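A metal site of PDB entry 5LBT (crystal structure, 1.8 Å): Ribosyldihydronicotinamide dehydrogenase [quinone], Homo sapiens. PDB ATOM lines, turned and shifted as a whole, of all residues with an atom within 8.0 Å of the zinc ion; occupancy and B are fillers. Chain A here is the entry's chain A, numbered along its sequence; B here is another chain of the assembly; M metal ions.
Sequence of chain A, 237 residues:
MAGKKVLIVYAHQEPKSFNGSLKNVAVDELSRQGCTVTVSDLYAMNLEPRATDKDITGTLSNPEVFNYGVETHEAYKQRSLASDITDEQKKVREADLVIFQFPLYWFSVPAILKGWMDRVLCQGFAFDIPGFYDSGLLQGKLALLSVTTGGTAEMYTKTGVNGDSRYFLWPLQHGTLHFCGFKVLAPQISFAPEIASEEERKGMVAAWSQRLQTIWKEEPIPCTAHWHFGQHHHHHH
The zinc ion is bound by ND1 of His 174 (2.1 Å), O of Cys 223 (2.2 Å), ND1 of His 178 (2.2 Å) and SG of Cys 223 (2.4 Å).
The zinc ion has four donor atoms within binding distance.
Of the 21 residues printed, 3 come within 4 Å of the zinc ion.
A ring nitrogen (NE2) of His 174 lies within hydrogen-bond range of the side-chain hydroxyl (OH) of Tyr 133, at 3.2 Å.
The backbone carbonyl oxygen (O) of His 174 sits at hydrogen-bond distance from the backbone NH (N) of Phe 179 (3.2 Å).
NE2 of His 174 is in hydrogen-bond range of O of Val 161 of chain B (3.2 Å).
The side-chain sulfur of Cys 223 sits close to the backbone carbonyl oxygen of Gln 173.
The backbone NH of His 178 is in hydrogen-bond range of the backbone carbonyl oxygen of Gln 173, at 2.7 Å.
The side-chain carboxylate of Asp 134 is in hydrogen-bond range of a ring nitrogen (NE2) of His 178 (2.6 Å).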
ATOM      1  N   TYR A 133      22.679   0.037 -10.517  1.00  0.00           N
ATOM      2  CA  TYR A 133      23.359   1.262 -10.852  1.00  0.00           C
ATOM      3  C   TYR A 133      22.449   2.119 -11.750  1.00  0.00           C
ATOM      4  O   TYR A 133      21.295   2.294 -11.373  1.00  0.00           O
ATOM      5  CB  TYR A 133      24.791   1.027 -11.339  1.00  0.00           C
ATOM      6  CG  TYR A 133      25.645   0.619 -10.154  1.00  0.00           C
ATOM      7  CD1 TYR A 133      25.703   1.401  -8.998  1.00  0.00           C
ATOM      8  CD2 TYR A 133      26.328  -0.587 -10.140  1.00  0.00           C
ATOM      9  CE1 TYR A 133      26.452   1.025  -7.877  1.00  0.00           C
ATOM     10  CE2 TYR A 133      27.052  -0.978  -9.033  1.00  0.00           C
ATOM     11  CZ  TYR A 133      27.118  -0.155  -7.916  1.00  0.00           C
ATOM     12  OH  TYR A 133      27.844  -0.525  -6.802  1.00  0.00           O
ATOM     13  N   ASP A 134      22.893   2.589 -12.918  1.00  0.00           N
ATOM     14  CA  ASP A 134      22.029   3.430 -13.762  1.00  0.00           C
ATOM     15  C   ASP A 134      20.702   2.768 -14.203  1.00  0.00           C
ATOM     16  O   ASP A 134      19.725   3.492 -14.453  1.00  0.00           O
ATOM     17  CB  ASP A 134      22.808   3.966 -14.976  1.00  0.00           C
ATOM     18  CG  ASP A 134      23.862   5.073 -14.605  1.00  0.00           C
ATOM     19  OD1 ASP A 134      24.047   5.415 -13.430  1.00  0.00           O
ATOM     20  OD2 ASP A 134      24.498   5.602 -15.554  1.00  0.00           O
ATOM     21  N   TRP A 170      30.312   7.077   0.392  1.00  0.00           N
ATOM     22  CA  TRP A 170      30.367   6.031  -0.669  1.00  0.00           C
ATOM     23  C   TRP A 170      29.395   4.881  -0.498  1.00  0.00           C
ATOM     24  O   TRP A 170      28.650   4.595  -1.440  1.00  0.00           O
ATOM     25  CB  TRP A 170      31.788   5.552  -0.826  1.00  0.00           C
ATOM     26  CG  TRP A 170      32.019   4.412  -1.712  1.00  0.00           C
ATOM     27  CD1 TRP A 170      32.320   3.166  -1.344  1.00  0.00           C
ATOM     28  CD2 TRP A 170      32.057   4.440  -3.131  1.00  0.00           C
ATOM     29  NE1 TRP A 170      32.531   2.378  -2.456  1.00  0.00           N
ATOM     30  CE2 TRP A 170      32.382   3.140  -3.572  1.00  0.00           C
ATOM     31  CE3 TRP A 170      31.810   5.424  -4.071  1.00  0.00           C
ATOM     32  CZ2 TRP A 170      32.483   2.796  -4.936  1.00  0.00           C
ATOM     33  CZ3 TRP A 170      31.943   5.071  -5.449  1.00  0.00           C
ATOM     34  CH2 TRP A 170      32.250   3.779  -5.849  1.00  0.00           C
ATOM     35  N   LEU A 172      26.615   4.773   1.094  1.00  0.00           N
ATOM     36  CA  LEU A 172      25.237   5.299   1.051  1.00  0.00           C
ATOM     37  C   LEU A 172      24.854   5.753  -0.333  1.00  0.00           C
ATOM     38  O   LEU A 172      23.879   5.262  -0.909  1.00  0.00           O
ATOM     39  CB  LEU A 172      25.064   6.445   2.063  1.00  0.00           C
ATOM     40  CG  LEU A 172      25.448   6.085   3.508  1.00  0.00           C
ATOM     41  CD1 LEU A 172      25.465   7.258   4.441  1.00  0.00           C
ATOM     42  CD2 LEU A 172      24.504   4.999   4.039  1.00  0.00           C
ATOM     43  N   GLN A 173      25.651   6.662  -0.885  1.00  0.00           N
ATOM     44  CA  GLN A 173      25.383   7.284  -2.196  1.00  0.00           C
ATOM     45  C   GLN A 173      25.539   6.293  -3.332  1.00  0.00           C
ATOM     46  O   GLN A 173      24.642   6.172  -4.163  1.00  0.00           O
ATOM     47  CB  GLN A 173      26.254   8.528  -2.403  1.00  0.00           C
ATOM     48  CG  GLN A 173      25.933   9.632  -1.400  1.00  0.00           C
ATOM     49  CD  GLN A 173      26.550  11.023  -1.678  1.00  0.00           C
ATOM     50  OE1 GLN A 173      25.982  12.056  -1.300  1.00  0.00           O
ATOM     51  NE2 GLN A 173      27.675  11.052  -2.375  1.00  0.00           N
ATOM     52  N   HIS A 174      26.658   5.586  -3.375  1.00  0.00           N
ATOM     53  CA  HIS A 174      26.944   4.671  -4.443  1.00  0.00           C
ATOM     54  C   HIS A 174      26.435   3.263  -4.177  1.00  0.00           C
ATOM     55  O   HIS A 174      25.746   2.685  -5.014  1.00  0.00           O
ATOM     56  CB  HIS A 174      28.424   4.638  -4.774  1.00  0.00           C
ATOM     57  CG  HIS A 174      28.774   3.753  -5.929  1.00  0.00           C
ATOM     58  ND1 HIS A 174      28.652   4.167  -7.240  1.00  0.00           N
ATOM     59  CD2 HIS A 174      29.261   2.485  -5.986  1.00  0.00           C
ATOM     60  CE1 HIS A 174      29.045   3.193  -8.051  1.00  0.00           C
ATOM     61  NE2 HIS A 174      29.420   2.165  -7.318  1.00  0.00           N
ATOM     62  N   GLY A 175      26.861   2.691  -3.054  1.00  0.00           N
ATOM     63  CA  GLY A 175      26.515   1.328  -2.723  1.00  0.00           C
ATOM     64  C   GLY A 175      25.021   1.068  -2.533  1.00  0.00           C
ATOM     65  O   GLY A 175      24.589  -0.036  -2.759  1.00  0.00           O
ATOM     66  N   THR A 176      24.247   2.106  -2.194  1.00  0.00           N
ATOM     67  CA  THR A 176      22.837   1.952  -1.917  1.00  0.00           C
ATOM     68  C   THR A 176      21.998   2.737  -2.942  1.00  0.00           C
ATOM     69  O   THR A 176      21.252   2.126  -3.729  1.00  0.00           O
ATOM     70  CB  THR A 176      22.486   2.397  -0.463  1.00  0.00           C
ATOM     71  OG1 THR A 176      23.352   1.773   0.481  1.00  0.00           O
ATOM     72  CG2 THR A 176      21.055   2.007  -0.072  1.00  0.00           C
ATOM     73  N   LEU A 177      22.100   4.080  -2.911  1.00  0.00           N
ATOM     74  CA  LEU A 177      21.220   4.919  -3.686  1.00  0.00           C
ATOM     75  C   LEU A 177      21.450   4.799  -5.217  1.00  0.00           C
ATOM     76  O   LEU A 177      20.508   4.524  -5.982  1.00  0.00           O
ATOM     77  CB  LEU A 177      21.313   6.361  -3.183  1.00  0.00           C
ATOM     78  CG  LEU A 177      20.929   6.585  -1.694  1.00  0.00           C
ATOM     79  CD1 LEU A 177      21.117   7.998  -1.303  1.00  0.00           C
ATOM     80  CD2 LEU A 177      19.494   6.201  -1.362  1.00  0.00           C
ATOM     81  N   HIS A 178      22.679   4.983  -5.673  1.00  0.00           N
ATOM     82  CA  HIS A 178      22.976   4.749  -7.080  1.00  0.00           C
ATOM     83  C   HIS A 178      22.677   3.314  -7.498  1.00  0.00           C
ATOM     84  O   HIS A 178      22.133   3.090  -8.571  1.00  0.00           O
ATOM     85  CB  HIS A 178      24.407   5.149  -7.357  1.00  0.00           C
ATOM     86  CG  HIS A 178      24.801   5.149  -8.793  1.00  0.00           C
ATOM     87  ND1 HIS A 178      26.108   5.205  -9.187  1.00  0.00           N
ATOM     88  CD2 HIS A 178      24.060   5.011  -9.925  1.00  0.00           C
ATOM     89  CE1 HIS A 178      26.172   5.145 -10.501  1.00  0.00           C
ATOM     90  NE2 HIS A 178      24.944   5.047 -10.973  1.00  0.00           N
ATOM     91  N   PHE A 179      22.980   2.336  -6.628  1.00  0.00           N
ATOM     92  CA  PHE A 179      22.763   0.950  -6.959  1.00  0.00           C
ATOM     93  C   PHE A 179      21.310   0.674  -7.317  1.00  0.00           C
ATOM     94  O   PHE A 179      21.046  -0.128  -8.214  1.00  0.00           O
ATOM     95  CB  PHE A 179      23.182   0.037  -5.799  1.00  0.00           C
ATOM     96  CG  PHE A 179      23.167  -1.412  -6.159  1.00  0.00           C
ATOM     97  CD1 PHE A 179      24.268  -1.983  -6.749  1.00  0.00           C
ATOM     98  CD2 PHE A 179      22.052  -2.218  -5.929  1.00  0.00           C
ATOM     99  CE1 PHE A 179      24.256  -3.340  -7.102  1.00  0.00           C
ATOM    100  CE2 PHE A 179      22.041  -3.548  -6.261  1.00  0.00           C
ATOM    101  CZ  PHE A 179      23.132  -4.111  -6.872  1.00  0.00           C
ATOM    102  N   PHE A 182      18.852   5.612  -8.179  1.00  0.00           N
ATOM    103  CA  PHE A 182      18.620   7.009  -7.826  1.00  0.00           C
ATOM    104  C   PHE A 182      19.692   7.895  -8.443  1.00  0.00           C
ATOM    105  O   PHE A 182      20.812   7.463  -8.652  1.00  0.00           O
ATOM    106  CB  PHE A 182      18.731   7.238  -6.326  1.00  0.00           C
ATOM    107  CG  PHE A 182      17.552   6.791  -5.513  1.00  0.00           C
ATOM    108  CD1 PHE A 182      16.418   7.550  -5.432  1.00  0.00           C
ATOM    109  CD2 PHE A 182      17.615   5.624  -4.770  1.00  0.00           C
ATOM    110  CE1 PHE A 182      15.354   7.156  -4.668  1.00  0.00           C
ATOM    111  CE2 PHE A 182      16.561   5.230  -3.996  1.00  0.00           C
ATOM    112  CZ  PHE A 182      15.420   5.992  -3.949  1.00  0.00           C
ATOM    113  N   VAL A 184      21.705  11.098  -7.413  1.00  0.00           N
ATOM    114  CA  VAL A 184      22.036  11.555  -6.104  1.00  0.00           C
ATOM    115  C   VAL A 184      22.294  13.047  -6.187  1.00  0.00           C
ATOM    116  O   VAL A 184      23.189  13.475  -6.896  1.00  0.00           O
ATOM    117  CB  VAL A 184      23.277  10.819  -5.566  1.00  0.00           C
ATOM    118  CG1 VAL A 184      23.661  11.283  -4.149  1.00  0.00           C
ATOM    119  CG2 VAL A 184      22.999   9.317  -5.545  1.00  0.00           C
ATOM    120  N   ILE A 221      24.981  14.736  -8.746  1.00  0.00           N
ATOM    121  CA  ILE A 221      26.418  14.576  -8.796  1.00  0.00           C
ATOM    122  C   ILE A 221      26.771  13.392  -9.687  1.00  0.00           C
ATOM    123  O   ILE A 221      25.931  12.552  -9.954  1.00  0.00           O
ATOM    124  CB  ILE A 221      27.010  14.262  -7.395  1.00  0.00           C
ATOM    125  CG1 ILE A 221      26.487  12.933  -6.876  1.00  0.00           C
ATOM    126  CG2 ILE A 221      26.707  15.376  -6.401  1.00  0.00           C
ATOM    127  CD1 ILE A 221      27.354  12.296  -5.809  1.00  0.00           C
ATOM    128  N   PRO A 222      28.080  13.358 -10.167  1.00  0.00           N
ATOM    129  CA  PRO A 222      28.401  12.147 -10.912  1.00  0.00           C
ATOM    130  C   PRO A 222      28.808  11.174  -9.791  1.00  0.00           C
ATOM    131  O   PRO A 222      29.828  11.378  -9.161  1.00  0.00           O
ATOM    132  CB  PRO A 222      29.570  12.557 -11.797  1.00  0.00           C
ATOM    133  CG  PRO A 222      30.276  13.628 -11.069  1.00  0.00           C
ATOM    134  CD  PRO A 222      29.291  14.292 -10.169  1.00  0.00           C
ATOM    135  N   CYS A 223      28.002  10.147  -9.549  1.00  0.00           N
ATOM    136  CA  CYS A 223      28.255   9.209  -8.440  1.00  0.00           C
ATOM    137  C   CYS A 223      29.268   8.151  -8.836  1.00  0.00           C
ATOM    138  O   CYS A 223      28.951   7.013  -9.112  1.00  0.00           O
ATOM    139  CB  CYS A 223      26.938   8.605  -7.944  1.00  0.00           C
ATOM    140  SG  CYS A 223      27.036   7.724  -6.373  1.00  0.00           S
ATOM    141  N   THR A 224      30.506   8.578  -8.817  1.00  0.00           N
ATOM    142  CA  THR A 224      31.608   7.734  -9.265  1.00  0.00           C
ATOM    143  C   THR A 224      32.599   7.538  -8.131  1.00  0.00           C
ATOM    144  O   THR A 224      32.619   8.304  -7.193  1.00  0.00           O
ATOM    145  CB  THR A 224      32.314   8.369 -10.473  1.00  0.00           C
ATOM    146  OG1 THR A 224      32.898   9.630 -10.099  1.00  0.00           O
ATOM    147  CG2 THR A 224      31.326   8.590 -11.641  1.00  0.00           C
ATOM    148  N   ALA A 225      33.440   6.498  -8.253  1.00  0.00           N
ATOM    149  CA  ALA A 225      34.606   6.362  -7.387  1.00  0.00           C
ATOM    150  C   ALA A 225      35.450   7.659  -7.442  1.00  0.00           C
ATOM    151  O   ALA A 225      35.867   8.188  -6.399  1.00  0.00           O
ATOM    152  CB  ALA A 225      35.435   5.126  -7.754  1.00  0.00           C
ATOM    153  N   TRP A 227      34.502  10.742  -7.942  1.00  0.00           N
ATOM    154  CA  TRP A 227      33.888  11.827  -7.165  1.00  0.00           C
ATOM    155  C   TRP A 227      34.172  11.658  -5.665  1.00  0.00           C
ATOM    156  O   TRP A 227      34.448  12.646  -4.955  1.00  0.00           O
ATOM    157  CB  TRP A 227      32.371  11.861  -7.341  1.00  0.00           C
ATOM    158  CG  TRP A 227      31.723  13.059  -6.713  1.00  0.00           C
ATOM    159  CD1 TRP A 227      31.503  14.287  -7.300  1.00  0.00           C
ATOM    160  CD2 TRP A 227      31.155  13.135  -5.412  1.00  0.00           C
ATOM    161  NE1 TRP A 227      30.845  15.093  -6.426  1.00  0.00           N
ATOM    162  CE2 TRP A 227      30.611  14.424  -5.265  1.00  0.00           C
ATOM    163  CE3 TRP A 227      31.055  12.233  -4.352  1.00  0.00           C
ATOM    164  CZ2 TRP A 227      30.022  14.839  -4.084  1.00  0.00           C
ATOM    165  CZ3 TRP A 227      30.467  12.657  -3.182  1.00  0.00           C
ATOM    166  CH2 TRP A 227      29.938  13.956  -3.061  1.00  0.00           C
ATOM    167  N   HIS A 228      34.061  10.420  -5.212  1.00  0.00           N
ATOM    168  CA  HIS A 228      34.224  10.139  -3.779  1.00  0.00           C
ATOM    169  C   HIS A 228      35.673  10.158  -3.294  1.00  0.00           C
ATOM    170  O   HIS A 228      35.924  10.623  -2.199  1.00  0.00           O
ATOM    171  CB  HIS A 228      33.560   8.831  -3.389  1.00  0.00           C
ATOM    172  CG  HIS A 228      32.061   8.866  -3.492  1.00  0.00           C
ATOM    173  ND1 HIS A 228      31.409   8.797  -4.706  1.00  0.00           N
ATOM    174  CD2 HIS A 228      31.097   8.991  -2.543  1.00  0.00           C
ATOM    175  CE1 HIS A 228      30.103   8.838  -4.487  1.00  0.00           C
ATOM    176  NE2 HIS A 228      29.887   8.977  -3.188  1.00  0.00           N
ATOM    177  N   VAL B 161      32.109  -2.517 -11.291  1.00  0.00           N
ATOM    178  CA  VAL B 161      30.919  -1.711 -10.976  1.00  0.00           C
ATOM    179  C   VAL B 161      30.851  -1.261  -9.503  1.00  0.00           C
ATOM    180  O   VAL B 161      30.378  -0.178  -9.246  1.00  0.00           O
ATOM    181  CB  VAL B 161      29.595  -2.405 -11.379  1.00  0.00           C
ATOM    182  CG1 VAL B 161      29.540  -2.592 -12.887  1.00  0.00           C
ATOM    183  CG2 VAL B 161      29.372  -3.714 -10.642  1.00  0.00           C
HETATM  184 ZN    ZN M   1      27.615   5.925  -7.784  1.00  0.00          ZN
